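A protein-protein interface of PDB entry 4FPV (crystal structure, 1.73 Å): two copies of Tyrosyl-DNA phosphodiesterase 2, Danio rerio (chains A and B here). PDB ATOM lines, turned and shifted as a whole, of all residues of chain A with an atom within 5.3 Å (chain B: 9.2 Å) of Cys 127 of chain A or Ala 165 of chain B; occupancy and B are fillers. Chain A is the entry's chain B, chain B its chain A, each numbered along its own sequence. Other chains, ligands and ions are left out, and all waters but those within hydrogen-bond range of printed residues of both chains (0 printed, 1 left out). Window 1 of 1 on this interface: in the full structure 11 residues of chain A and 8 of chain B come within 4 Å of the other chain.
The side-chain amide nitrogen (ND2) of Asn 169 of chain B lies close to the backbone carbonyl oxygen (O) of Ala 165 of chain B.
SD of Met 101 of chain A sits at hydrogen-bond distance from N of Ser 126 of chain A, 3.5 Å away.
The backbone carbonyl oxygen (O) of Cys 127 of chain A lies within hydrogen-bond range of the guanidinium group (NH1) of Arg 134 of chain A, at 2.8 Å.
Printed residues of chain B within 4 Å of Cys 127 of chain A: Ala 165 (3.4 Å).
Of the printed residues of chain A, Asp 164 of chain B touches Asn 129 (2.9 Å) and Gln 130 (2.6 Å).
Of the printed residues of chain A, Asn 169 of chain B touches Met 101 (3.9 Å).
Of the printed residues of chain B, Met 101 of chain A touches Ala 165 and Asn 169.
Printed residues of chain B within 4 Å of Gln 130 of chain A: Asp 164 (2.6 Å).
Of the printed residues of chain B, Asn 129 of chain A touches Asp 164 (2.9 Å).
The nearest printed residue of chain A that does not touch Ala 165 of chain B is Ser 126 of chain A (4.005 Å).
The nearest printed residue of chain B that does not touch Gln 130 of chain A is Ala 165 of chain B (6.1 Å).
Among the printed residues, pairs that only touch across the chains: Met 101 of chain A with Ala 165 of chain B (3.7 Å) and Met 101 of chain A with Asn 169 of chain B (3.9 Å).
The side-chain amide nitrogen (ND2) of Asn 129 of chain A lies close to the side-chain carboxylate (OD1) of Asp 164 of chain B (2.9 Å).
NE2 of Gln 130 of chain A is in hydrogen-bond range of OD2 of Asp 164 of chain B (2.6 Å).
N of Ala 165 of chain B sits at hydrogen-bond distance from SG of Cys 127 of chain A (3.4 Å).
Positions printed for both chains: 131, 134 and 163.
Of the 5 pairs that touch across the chains among the printed residues, none has its exchanged pair printed and touching as well.
Hydrophobic or aromatic side chains of chain B that line the printed part of chain A: Ala 165.
Printed residues of chain A that touch a printed residue of chain B: Met 101, Cys 127, Asn 129 and Gln 130.
Along chain A the printed residues that touch a printed residue of chain B span positions 101 to 130.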
ATOM      1  N   MET A 101      23.132 -27.458   1.386  1.00  0.00           N
ATOM      2  CA  MET A 101      22.702 -27.767   0.033  1.00  0.00           C
ATOM      3  C   MET A 101      23.549 -28.875  -0.580  1.00  0.00           C
ATOM      4  O   MET A 101      23.591 -29.013  -1.804  1.00  0.00           O
ATOM      5  CB  MET A 101      22.766 -26.508  -0.828  1.00  0.00           C
ATOM      6  CG  MET A 101      22.142 -25.299  -0.158  1.00  0.00           C
ATOM      7  SD  MET A 101      22.089 -23.869  -1.239  1.00  0.00           S
ATOM      8  CE  MET A 101      21.697 -22.574  -0.049  1.00  0.00           C
ATOM      9  N   GLU A 125      27.498 -22.517  -2.449  1.00  0.00           N
ATOM     10  CA  GLU A 125      26.194 -22.235  -1.825  1.00  0.00           C
ATOM     11  C   GLU A 125      25.400 -21.188  -2.602  1.00  0.00           C
ATOM     12  O   GLU A 125      25.944 -20.130  -2.959  1.00  0.00           O
ATOM     13  CB  GLU A 125      26.402 -21.765  -0.388  1.00  0.00           C
ATOM     14  CG  GLU A 125      25.223 -22.116   0.534  1.00  0.00           C
ATOM     15  CD  GLU A 125      25.202 -23.575   0.970  1.00  0.00           C
ATOM     16  OE1 GLU A 125      26.011 -24.394   0.476  1.00  0.00           O
ATOM     17  OE2 GLU A 125      24.365 -23.912   1.835  1.00  0.00           O
ATOM     18  N   SER A 126      24.133 -21.506  -2.880  1.00  0.00           N
ATOM     19  CA  SER A 126      23.282 -20.712  -3.752  1.00  0.00           C
ATOM     20  C   SER A 126      22.582 -19.581  -3.017  1.00  0.00           C
ATOM     21  O   SER A 126      22.410 -19.636  -1.784  1.00  0.00           O
ATOM     22  CB  SER A 126      22.221 -21.600  -4.420  1.00  0.00           C
ATOM     23  OG  SER A 126      22.806 -22.617  -5.208  1.00  0.00           O
ATOM     24  N   CYS A 127      22.195 -18.572  -3.800  1.00  0.00           N
ATOM     25  CA  CYS A 127      21.347 -17.455  -3.365  1.00  0.00           C
ATOM     26  C   CYS A 127      22.095 -16.297  -2.699  1.00  0.00           C
ATOM     27  O   CYS A 127      23.043 -16.498  -1.953  1.00  0.00           O
ATOM     28  CB  CYS A 127      20.187 -17.959  -2.502  1.00  0.00           C
ATOM     29  SG  CYS A 127      19.085 -19.062  -3.395  1.00  0.00           S
ATOM     30  N   LYS A 128      21.657 -15.071  -2.986  1.00  0.00           N
ATOM     31  CA  LYS A 128      22.347 -13.863  -2.508  1.00  0.00           C
ATOM     32  C   LYS A 128      22.530 -13.874  -0.993  1.00  0.00           C
ATOM     33  O   LYS A 128      23.613 -13.625  -0.442  1.00  0.00           O
ATOM     34  CB  LYS A 128      21.568 -12.630  -2.962  1.00  0.00           C
ATOM     35  CG  LYS A 128      22.010 -11.313  -2.350  1.00  0.00           C
ATOM     36  CD  LYS A 128      21.092 -10.195  -2.838  1.00  0.00           C
ATOM     37  CE  LYS A 128      21.039  -9.026  -1.864  1.00  0.00           C
ATOM     38  NZ  LYS A 128      22.310  -8.252  -1.859  1.00  0.00           N
ATOM     39  N   ASN A 129      21.445 -14.248  -0.334  1.00  0.00           N
ATOM     40  CA  ASN A 129      21.341 -14.325   1.114  1.00  0.00           C
ATOM     41  C   ASN A 129      22.337 -15.297   1.760  1.00  0.00           C
ATOM     42  O   ASN A 129      22.558 -15.268   2.974  1.00  0.00           O
ATOM     43  CB  ASN A 129      19.906 -14.768   1.363  1.00  0.00           C
ATOM     44  CG  ASN A 129      19.148 -14.984   0.031  1.00  0.00           C
ATOM     45  OD1 ASN A 129      18.800 -14.030  -0.667  1.00  0.00           O
ATOM     46  ND2 ASN A 129      18.955 -16.232  -0.344  1.00  0.00           N
ATOM     47  N   GLN A 130      22.956 -16.151   0.947  1.00  0.00           N
ATOM     48  CA  GLN A 130      23.920 -17.109   1.483  1.00  0.00           C
ATOM     49  C   GLN A 130      25.360 -16.665   1.254  1.00  0.00           C
ATOM     50  O   GLN A 130      26.301 -17.486   1.310  1.00  0.00           O
ATOM     51  CB  GLN A 130      23.667 -18.509   0.924  1.00  0.00           C
ATOM     52  CG  GLN A 130      22.386 -19.146   1.466  1.00  0.00           C
ATOM     53  CD  GLN A 130      22.375 -19.227   2.987  1.00  0.00           C
ATOM     54  OE1 GLN A 130      23.342 -19.663   3.603  1.00  0.00           O
ATOM     55  NE2 GLN A 130      21.275 -18.791   3.599  1.00  0.00           N
ATOM     56  N   SER A 131      25.530 -15.355   1.040  1.00  0.00           N
ATOM     57  CA  SER A 131      26.879 -14.786   0.922  1.00  0.00           C
ATOM     58  C   SER A 131      27.890 -15.323   1.949  1.00  0.00           C
ATOM     59  O   SER A 131      29.043 -15.581   1.615  1.00  0.00           O
ATOM     60  CB  SER A 131      26.835 -13.251   0.999  1.00  0.00           C
ATOM     61  OG  SER A 131      28.148 -12.727   0.935  1.00  0.00           O
ATOM     62  N   ARG A 134      28.726 -19.160   1.209  1.00  0.00           N
ATOM     63  CA  ARG A 134      29.407 -19.161  -0.082  1.00  0.00           C
ATOM     64  C   ARG A 134      30.832 -18.662   0.097  1.00  0.00           C
ATOM     65  O   ARG A 134      31.788 -19.286  -0.405  1.00  0.00           O
ATOM     66  CB  ARG A 134      28.630 -18.302  -1.076  1.00  0.00           C
ATOM     67  CG  ARG A 134      29.318 -18.149  -2.423  1.00  0.00           C
ATOM     68  CD  ARG A 134      28.352 -17.610  -3.439  1.00  0.00           C
ATOM     69  NE  ARG A 134      27.734 -16.346  -3.022  1.00  0.00           N
ATOM     70  CZ  ARG A 134      26.448 -16.213  -2.683  1.00  0.00           C
ATOM     71  NH1 ARG A 134      25.640 -17.273  -2.675  1.00  0.00           N
ATOM     72  NH2 ARG A 134      25.972 -15.022  -2.328  1.00  0.00           N
ATOM     73  N   ASN A 161      28.324 -19.051  -7.969  1.00  0.00           N
ATOM     74  CA  ASN A 161      27.250 -18.188  -7.448  1.00  0.00           C
ATOM     75  C   ASN A 161      27.734 -16.861  -6.880  1.00  0.00           C
ATOM     76  O   ASN A 161      27.011 -16.189  -6.135  1.00  0.00           O
ATOM     77  CB  ASN A 161      26.420 -18.933  -6.388  1.00  0.00           C
ATOM     78  CG  ASN A 161      25.339 -19.786  -7.000  1.00  0.00           C
ATOM     79  OD1 ASN A 161      24.501 -19.300  -7.770  1.00  0.00           O
ATOM     80  ND2 ASN A 161      25.352 -21.071  -6.677  1.00  0.00           N
ATOM     81  N   ARG A 163      28.749 -12.987  -6.501  1.00  0.00           N
ATOM     82  CA  ARG A 163      28.273 -11.725  -7.026  1.00  0.00           C
ATOM     83  C   ARG A 163      29.182 -10.594  -6.629  1.00  0.00           C
ATOM     84  O   ARG A 163      30.248 -10.804  -6.040  1.00  0.00           O
ATOM     85  CB  ARG A 163      26.833 -11.438  -6.610  1.00  0.00           C
ATOM     86  CG  ARG A 163      26.522 -11.786  -5.190  1.00  0.00           C
ATOM     87  CD  ARG A 163      25.848 -13.129  -5.141  1.00  0.00           C
ATOM     88  NE  ARG A 163      24.492 -13.059  -5.672  1.00  0.00           N
ATOM     89  CZ  ARG A 163      23.744 -14.126  -5.931  1.00  0.00           C
ATOM     90  NH1 ARG A 163      22.512 -13.972  -6.409  1.00  0.00           N
ATOM     91  NH2 ARG A 163      24.234 -15.348  -5.719  1.00  0.00           N
ATOM     92  N   SER B 131      14.993 -30.107   5.289  1.00  0.00           N
ATOM     93  CA  SER B 131      14.892 -29.613   3.917  1.00  0.00           C
ATOM     94  C   SER B 131      14.501 -30.695   2.911  1.00  0.00           C
ATOM     95  O   SER B 131      13.766 -30.422   1.964  1.00  0.00           O
ATOM     96  CB  SER B 131      16.204 -28.946   3.493  1.00  0.00           C
ATOM     97  OG  SER B 131      17.289 -29.840   3.663  1.00  0.00           O
ATOM     98  N   ARG B 134      10.667 -31.423   3.514  1.00  0.00           N
ATOM     99  CA  ARG B 134      10.013 -30.170   3.150  1.00  0.00           C
ATOM    100  C   ARG B 134       9.996 -29.997   1.637  1.00  0.00           C
ATOM    101  O   ARG B 134       8.947 -29.666   1.046  1.00  0.00           O
ATOM    102  CB  ARG B 134      10.703 -28.993   3.852  1.00  0.00           C
ATOM    103  CG  ARG B 134      10.185 -27.636   3.465  1.00  0.00           C
ATOM    104  CD  ARG B 134      10.569 -26.601   4.520  1.00  0.00           C
ATOM    105  NE  ARG B 134      12.025 -26.451   4.651  1.00  0.00           N
ATOM    106  CZ  ARG B 134      12.728 -26.849   5.711  1.00  0.00           C
ATOM    107  NH1 ARG B 134      12.127 -27.442   6.746  1.00  0.00           N
ATOM    108  NH2 ARG B 134      14.048 -26.657   5.738  1.00  0.00           N
ATOM    109  N   THR B 135      11.121 -30.297   0.978  1.00  0.00           N
ATOM    110  CA  THR B 135      11.140 -30.028  -0.452  1.00  0.00           C
ATOM    111  C   THR B 135      10.269 -31.028  -1.191  1.00  0.00           C
ATOM    112  O   THR B 135       9.582 -30.658  -2.154  1.00  0.00           O
ATOM    113  CB  THR B 135      12.577 -29.917  -1.032  1.00  0.00           C
ATOM    114  OG1 THR B 135      13.365 -31.018  -0.590  1.00  0.00           O
ATOM    115  CG2 THR B 135      13.209 -28.643  -0.537  1.00  0.00           C
ATOM    116  N   LEU B 138       6.986 -29.684  -0.968  1.00  0.00           N
ATOM    117  CA  LEU B 138       6.767 -28.523  -1.813  1.00  0.00           C
ATOM    118  C   LEU B 138       6.469 -29.009  -3.226  1.00  0.00           C
ATOM    119  O   LEU B 138       5.589 -28.441  -3.910  1.00  0.00           O
ATOM    120  CB  LEU B 138       7.971 -27.566  -1.789  1.00  0.00           C
ATOM    121  CG  LEU B 138       7.963 -26.385  -2.763  1.00  0.00           C
ATOM    122  CD1 LEU B 138       6.877 -25.359  -2.419  1.00  0.00           C
ATOM    123  CD2 LEU B 138       9.337 -25.725  -2.761  1.00  0.00           C
ATOM    124  N   ARG B 139       7.144 -30.095  -3.632  1.00  0.00           N
ATOM    125  CA  ARG B 139       6.935 -30.602  -4.991  1.00  0.00           C
ATOM    126  C   ARG B 139       5.460 -30.900  -5.160  1.00  0.00           C
ATOM    127  O   ARG B 139       4.804 -30.397  -6.103  1.00  0.00           O
ATOM    128  CB  ARG B 139       7.780 -31.856  -5.258  1.00  0.00           C
ATOM    129  CG  ARG B 139       9.276 -31.587  -5.259  1.00  0.00           C
ATOM    130  CD  ARG B 139      10.115 -32.756  -5.788  1.00  0.00           C
ATOM    131  NE  ARG B 139      11.547 -32.446  -5.736  1.00  0.00           N
ATOM    132  CZ  ARG B 139      12.239 -31.932  -6.752  1.00  0.00           C
ATOM    133  NH1 ARG B 139      11.638 -31.675  -7.906  1.00  0.00           N
ATOM    134  NH2 ARG B 139      13.536 -31.673  -6.617  1.00  0.00           N
ATOM    135  N   LEU B 162      10.062 -22.482   4.296  1.00  0.00           N
ATOM    136  CA  LEU B 162      11.039 -22.526   3.206  1.00  0.00           C
ATOM    137  C   LEU B 162      12.237 -21.634   3.460  1.00  0.00           C
ATOM    138  O   LEU B 162      12.119 -20.516   3.992  1.00  0.00           O
ATOM    139  CB  LEU B 162      10.397 -22.159   1.862  1.00  0.00           C
ATOM    140  CG  LEU B 162       9.581 -23.301   1.255  1.00  0.00           C
ATOM    141  CD1 LEU B 162       8.740 -22.775   0.079  1.00  0.00           C
ATOM    142  CD2 LEU B 162      10.463 -24.490   0.819  1.00  0.00           C
ATOM    143  N   ARG B 163      13.400 -22.139   3.053  1.00  0.00           N
ATOM    144  CA  ARG B 163      14.652 -21.400   3.131  1.00  0.00           C
ATOM    145  C   ARG B 163      15.142 -20.930   1.784  1.00  0.00           C
ATOM    146  O   ARG B 163      14.559 -21.233   0.732  1.00  0.00           O
ATOM    147  CB  ARG B 163      15.762 -22.275   3.702  1.00  0.00           C
ATOM    148  CG  ARG B 163      16.074 -22.005   5.135  1.00  0.00           C
ATOM    149  CD  ARG B 163      14.992 -22.583   5.997  1.00  0.00           C
ATOM    150  NE  ARG B 163      15.284 -22.450   7.418  1.00  0.00           N
ATOM    151  CZ  ARG B 163      14.579 -23.049   8.368  1.00  0.00           C
ATOM    152  NH1 ARG B 163      13.543 -23.820   8.039  1.00  0.00           N
ATOM    153  NH2 ARG B 163      14.906 -22.879   9.643  1.00  0.00           N
ATOM    154  N   ASP B 164      16.248 -20.194   1.852  1.00  0.00           N
ATOM    155  CA  ASP B 164      17.058 -19.872   0.689  1.00  0.00           C
ATOM    156  C   ASP B 164      17.321 -21.107  -0.148  1.00  0.00           C
ATOM    157  O   ASP B 164      17.735 -22.152   0.374  1.00  0.00           O
ATOM    158  CB  ASP B 164      18.396 -19.295   1.134  1.00  0.00           C
ATOM    159  CG  ASP B 164      18.251 -17.970   1.832  1.00  0.00           C
ATOM    160  OD1 ASP B 164      17.200 -17.313   1.664  1.00  0.00           O
ATOM    161  OD2 ASP B 164      19.209 -17.572   2.519  1.00  0.00           O
ATOM    162  N   ALA B 165      17.057 -20.972  -1.444  1.00  0.00           N
ATOM    163  CA  ALA B 165      17.378 -21.980  -2.446  1.00  0.00           C
ATOM    164  C   ALA B 165      16.494 -23.215  -2.420  1.00  0.00           C
ATOM    165  O   ALA B 165      16.531 -24.001  -3.361  1.00  0.00           O
ATOM    166  CB  ALA B 165      18.868 -22.381  -2.374  1.00  0.00           C
ATOM    167  N   GLU B 166      15.701 -23.412  -1.369  1.00  0.00           N
ATOM    168  CA  GLU B 166      14.843 -24.599  -1.368  1.00  0.00           C
ATOM    169  C   GLU B 166      13.852 -24.585  -2.527  1.00  0.00           C
ATOM    170  O   GLU B 166      13.553 -25.636  -3.104  1.00  0.00           O
ATOM    171  CB  GLU B 166      14.174 -24.850  -0.001  1.00  0.00           C
ATOM    172  CG  GLU B 166      15.178 -25.259   1.077  1.00  0.00           C
ATOM    173  CD  GLU B 166      14.587 -25.407   2.485  1.00  0.00           C
ATOM    174  OE1 GLU B 166      13.435 -24.979   2.728  1.00  0.00           O
ATOM    175  OE2 GLU B 166      15.302 -25.935   3.369  1.00  0.00           O
ATOM    176  N   VAL B 167      13.372 -23.399  -2.901  1.00  0.00           N
ATOM    177  CA  VAL B 167      12.503 -23.302  -4.065  1.00  0.00           C
ATOM    178  C   VAL B 167      13.331 -23.462  -5.343  1.00  0.00           C
ATOM    179  O   VAL B 167      12.942 -24.186  -6.258  1.00  0.00           O
ATOM    180  CB  VAL B 167      11.702 -21.993  -4.085  1.00  0.00           C
ATOM    181  CG1 VAL B 167      10.843 -21.920  -5.330  1.00  0.00           C
ATOM    182  CG2 VAL B 167      10.821 -21.926  -2.839  1.00  0.00           C
ATOM    183  N   ALA B 168      14.475 -22.785  -5.394  1.00  0.00           N
ATOM    184  CA  ALA B 168      15.382 -22.924  -6.529  1.00  0.00           C
ATOM    185  C   ALA B 168      15.813 -24.384  -6.668  1.00  0.00           C
ATOM    186  O   ALA B 168      15.736 -24.959  -7.756  1.00  0.00           O
ATOM    187  CB  ALA B 168      16.592 -22.008  -6.371  1.00  0.00           C
ATOM    188  N   ASN B 169      16.229 -24.996  -5.562  1.00  0.00           N
ATOM    189  CA  ASN B 169      16.675 -26.391  -5.595  1.00  0.00           C
ATOM    190  C   ASN B 169      15.557 -27.398  -5.894  1.00  0.00           C
ATOM    191  O   ASN B 169      15.774 -28.607  -5.854  1.00  0.00           O
ATOM    192  CB  ASN B 169      17.428 -26.782  -4.310  1.00  0.00           C
ATOM    193  CG  ASN B 169      18.648 -25.903  -4.042  1.00  0.00           C
ATOM    194  OD1 ASN B 169      19.146 -25.214  -4.931  1.00  0.00           O
ATOM    195  ND2 ASN B 169      19.124 -25.922  -2.799  1.00  0.00           N
ATOM    196  N   VAL B 170      14.366 -26.897  -6.207  1.00  0.00           N
ATOM    197  CA  VAL B 170      13.278 -27.757  -6.672  1.00  0.00           C
ATOM    198  C   VAL B 170      12.967 -27.452  -8.145  1.00  0.00           C
ATOM    199  O   VAL B 170      12.096 -28.072  -8.758  1.00  0.00           O
ATOM    200  CB  VAL B 170      12.021 -27.620  -5.772  1.00  0.00           C
ATOM    201  CG1 VAL B 170      11.052 -26.556  -6.297  1.00  0.00           C
ATOM    202  CG2 VAL B 170      11.321 -28.931  -5.664  1.00  0.00           C
ATOM    203  N   GLY B 171      13.708 -26.510  -8.720  1.00  0.00           N
ATOM    204  CA  GLY B 171      13.497 -26.124 -10.105  1.00  0.00           C
ATOM    205  C   GLY B 171      12.759 -24.804 -10.259  1.00  0.00           C
ATOM    206  O   GLY B 171      12.404 -24.412 -11.379  1.00  0.00           O
ATOM    207  N   GLY B 172      12.531 -24.119  -9.137  1.00  0.00           N
ATOM    208  CA  GLY B 172      11.774 -22.876  -9.129  1.00  0.00           C
ATOM    209  C   GLY B 172      10.274 -23.116  -9.246  1.00  0.00           C
ATOM    210  O   GLY B 172       9.821 -24.245  -9.412  1.00  0.00           O
ATOM    211  N   ARG B 191       8.664  -8.391   4.245  1.00  0.00           N
ATOM    212  CA  ARG B 191       9.513  -9.549   3.911  1.00  0.00           C
ATOM    213  C   ARG B 191       9.529 -10.700   4.940  1.00  0.00           C
ATOM    214  O   ARG B 191       9.033 -11.805   4.663  1.00  0.00           O
ATOM    215  CB  ARG B 191      10.945  -9.081   3.637  1.00  0.00           C
ATOM    216  CG  ARG B 191      11.845 -10.196   3.151  1.00  0.00           C
ATOM    217  CD  ARG B 191      13.238  -9.687   2.836  1.00  0.00           C
ATOM    218  NE  ARG B 191      14.016 -10.720   2.160  1.00  0.00           N
ATOM    219  CZ  ARG B 191      15.319 -10.638   1.925  1.00  0.00           C
ATOM    220  NH1 ARG B 191      16.000  -9.565   2.314  1.00  0.00           N
ATOM    221  NH2 ARG B 191      15.941 -11.631   1.301  1.00  0.00           N
ATOM    222  N   ARG B 211      11.484 -15.848   5.861  1.00  0.00           N
ATOM    223  CA  ARG B 211      10.226 -15.677   5.128  1.00  0.00           C
ATOM    224  C   ARG B 211       9.561 -17.040   4.962  1.00  0.00           C
ATOM    225  O   ARG B 211       9.527 -17.608   3.869  1.00  0.00           O
ATOM    226  CB  ARG B 211      10.454 -15.017   3.763  1.00  0.00           C
ATOM    227  CG  ARG B 211       9.162 -14.532   3.106  1.00  0.00           C
ATOM    228  CD  ARG B 211       9.423 -13.632   1.893  1.00  0.00           C
ATOM    229  NE  ARG B 211      10.036 -14.359   0.784  1.00  0.00           N
ATOM    230  CZ  ARG B 211       9.357 -14.995  -0.171  1.00  0.00           C
ATOM    231  NH1 ARG B 211       8.031 -15.001  -0.154  1.00  0.00           N
ATOM    232  NH2 ARG B 211      10.000 -15.620  -1.148  1.00  0.00           N
ATOM    233  N   ARG B 214       4.255 -17.883   2.944  1.00  0.00           N
ATOM    234  CA  ARG B 214       4.214 -17.489   1.536  1.00  0.00           C
ATOM    235  C   ARG B 214       2.872 -17.772   0.887  1.00  0.00           C
ATOM    236  O   ARG B 214       2.109 -18.644   1.336  1.00  0.00           O
ATOM    237  CB  ARG B 214       5.323 -18.205   0.747  1.00  0.00           C
ATOM    238  CG  ARG B 214       6.704 -18.032   1.365  1.00  0.00           C
ATOM    239  CD  ARG B 214       7.811 -18.578   0.474  1.00  0.00           C
ATOM    240  NE  ARG B 214       9.101 -18.429   1.136  1.00  0.00           N
ATOM    241  CZ  ARG B 214      10.280 -18.643   0.561  1.00  0.00           C
ATOM    242  NH1 ARG B 214      10.350 -19.010  -0.714  1.00  0.00           N
ATOM    243  NH2 ARG B 214      11.387 -18.477   1.270  1.00  0.00           N
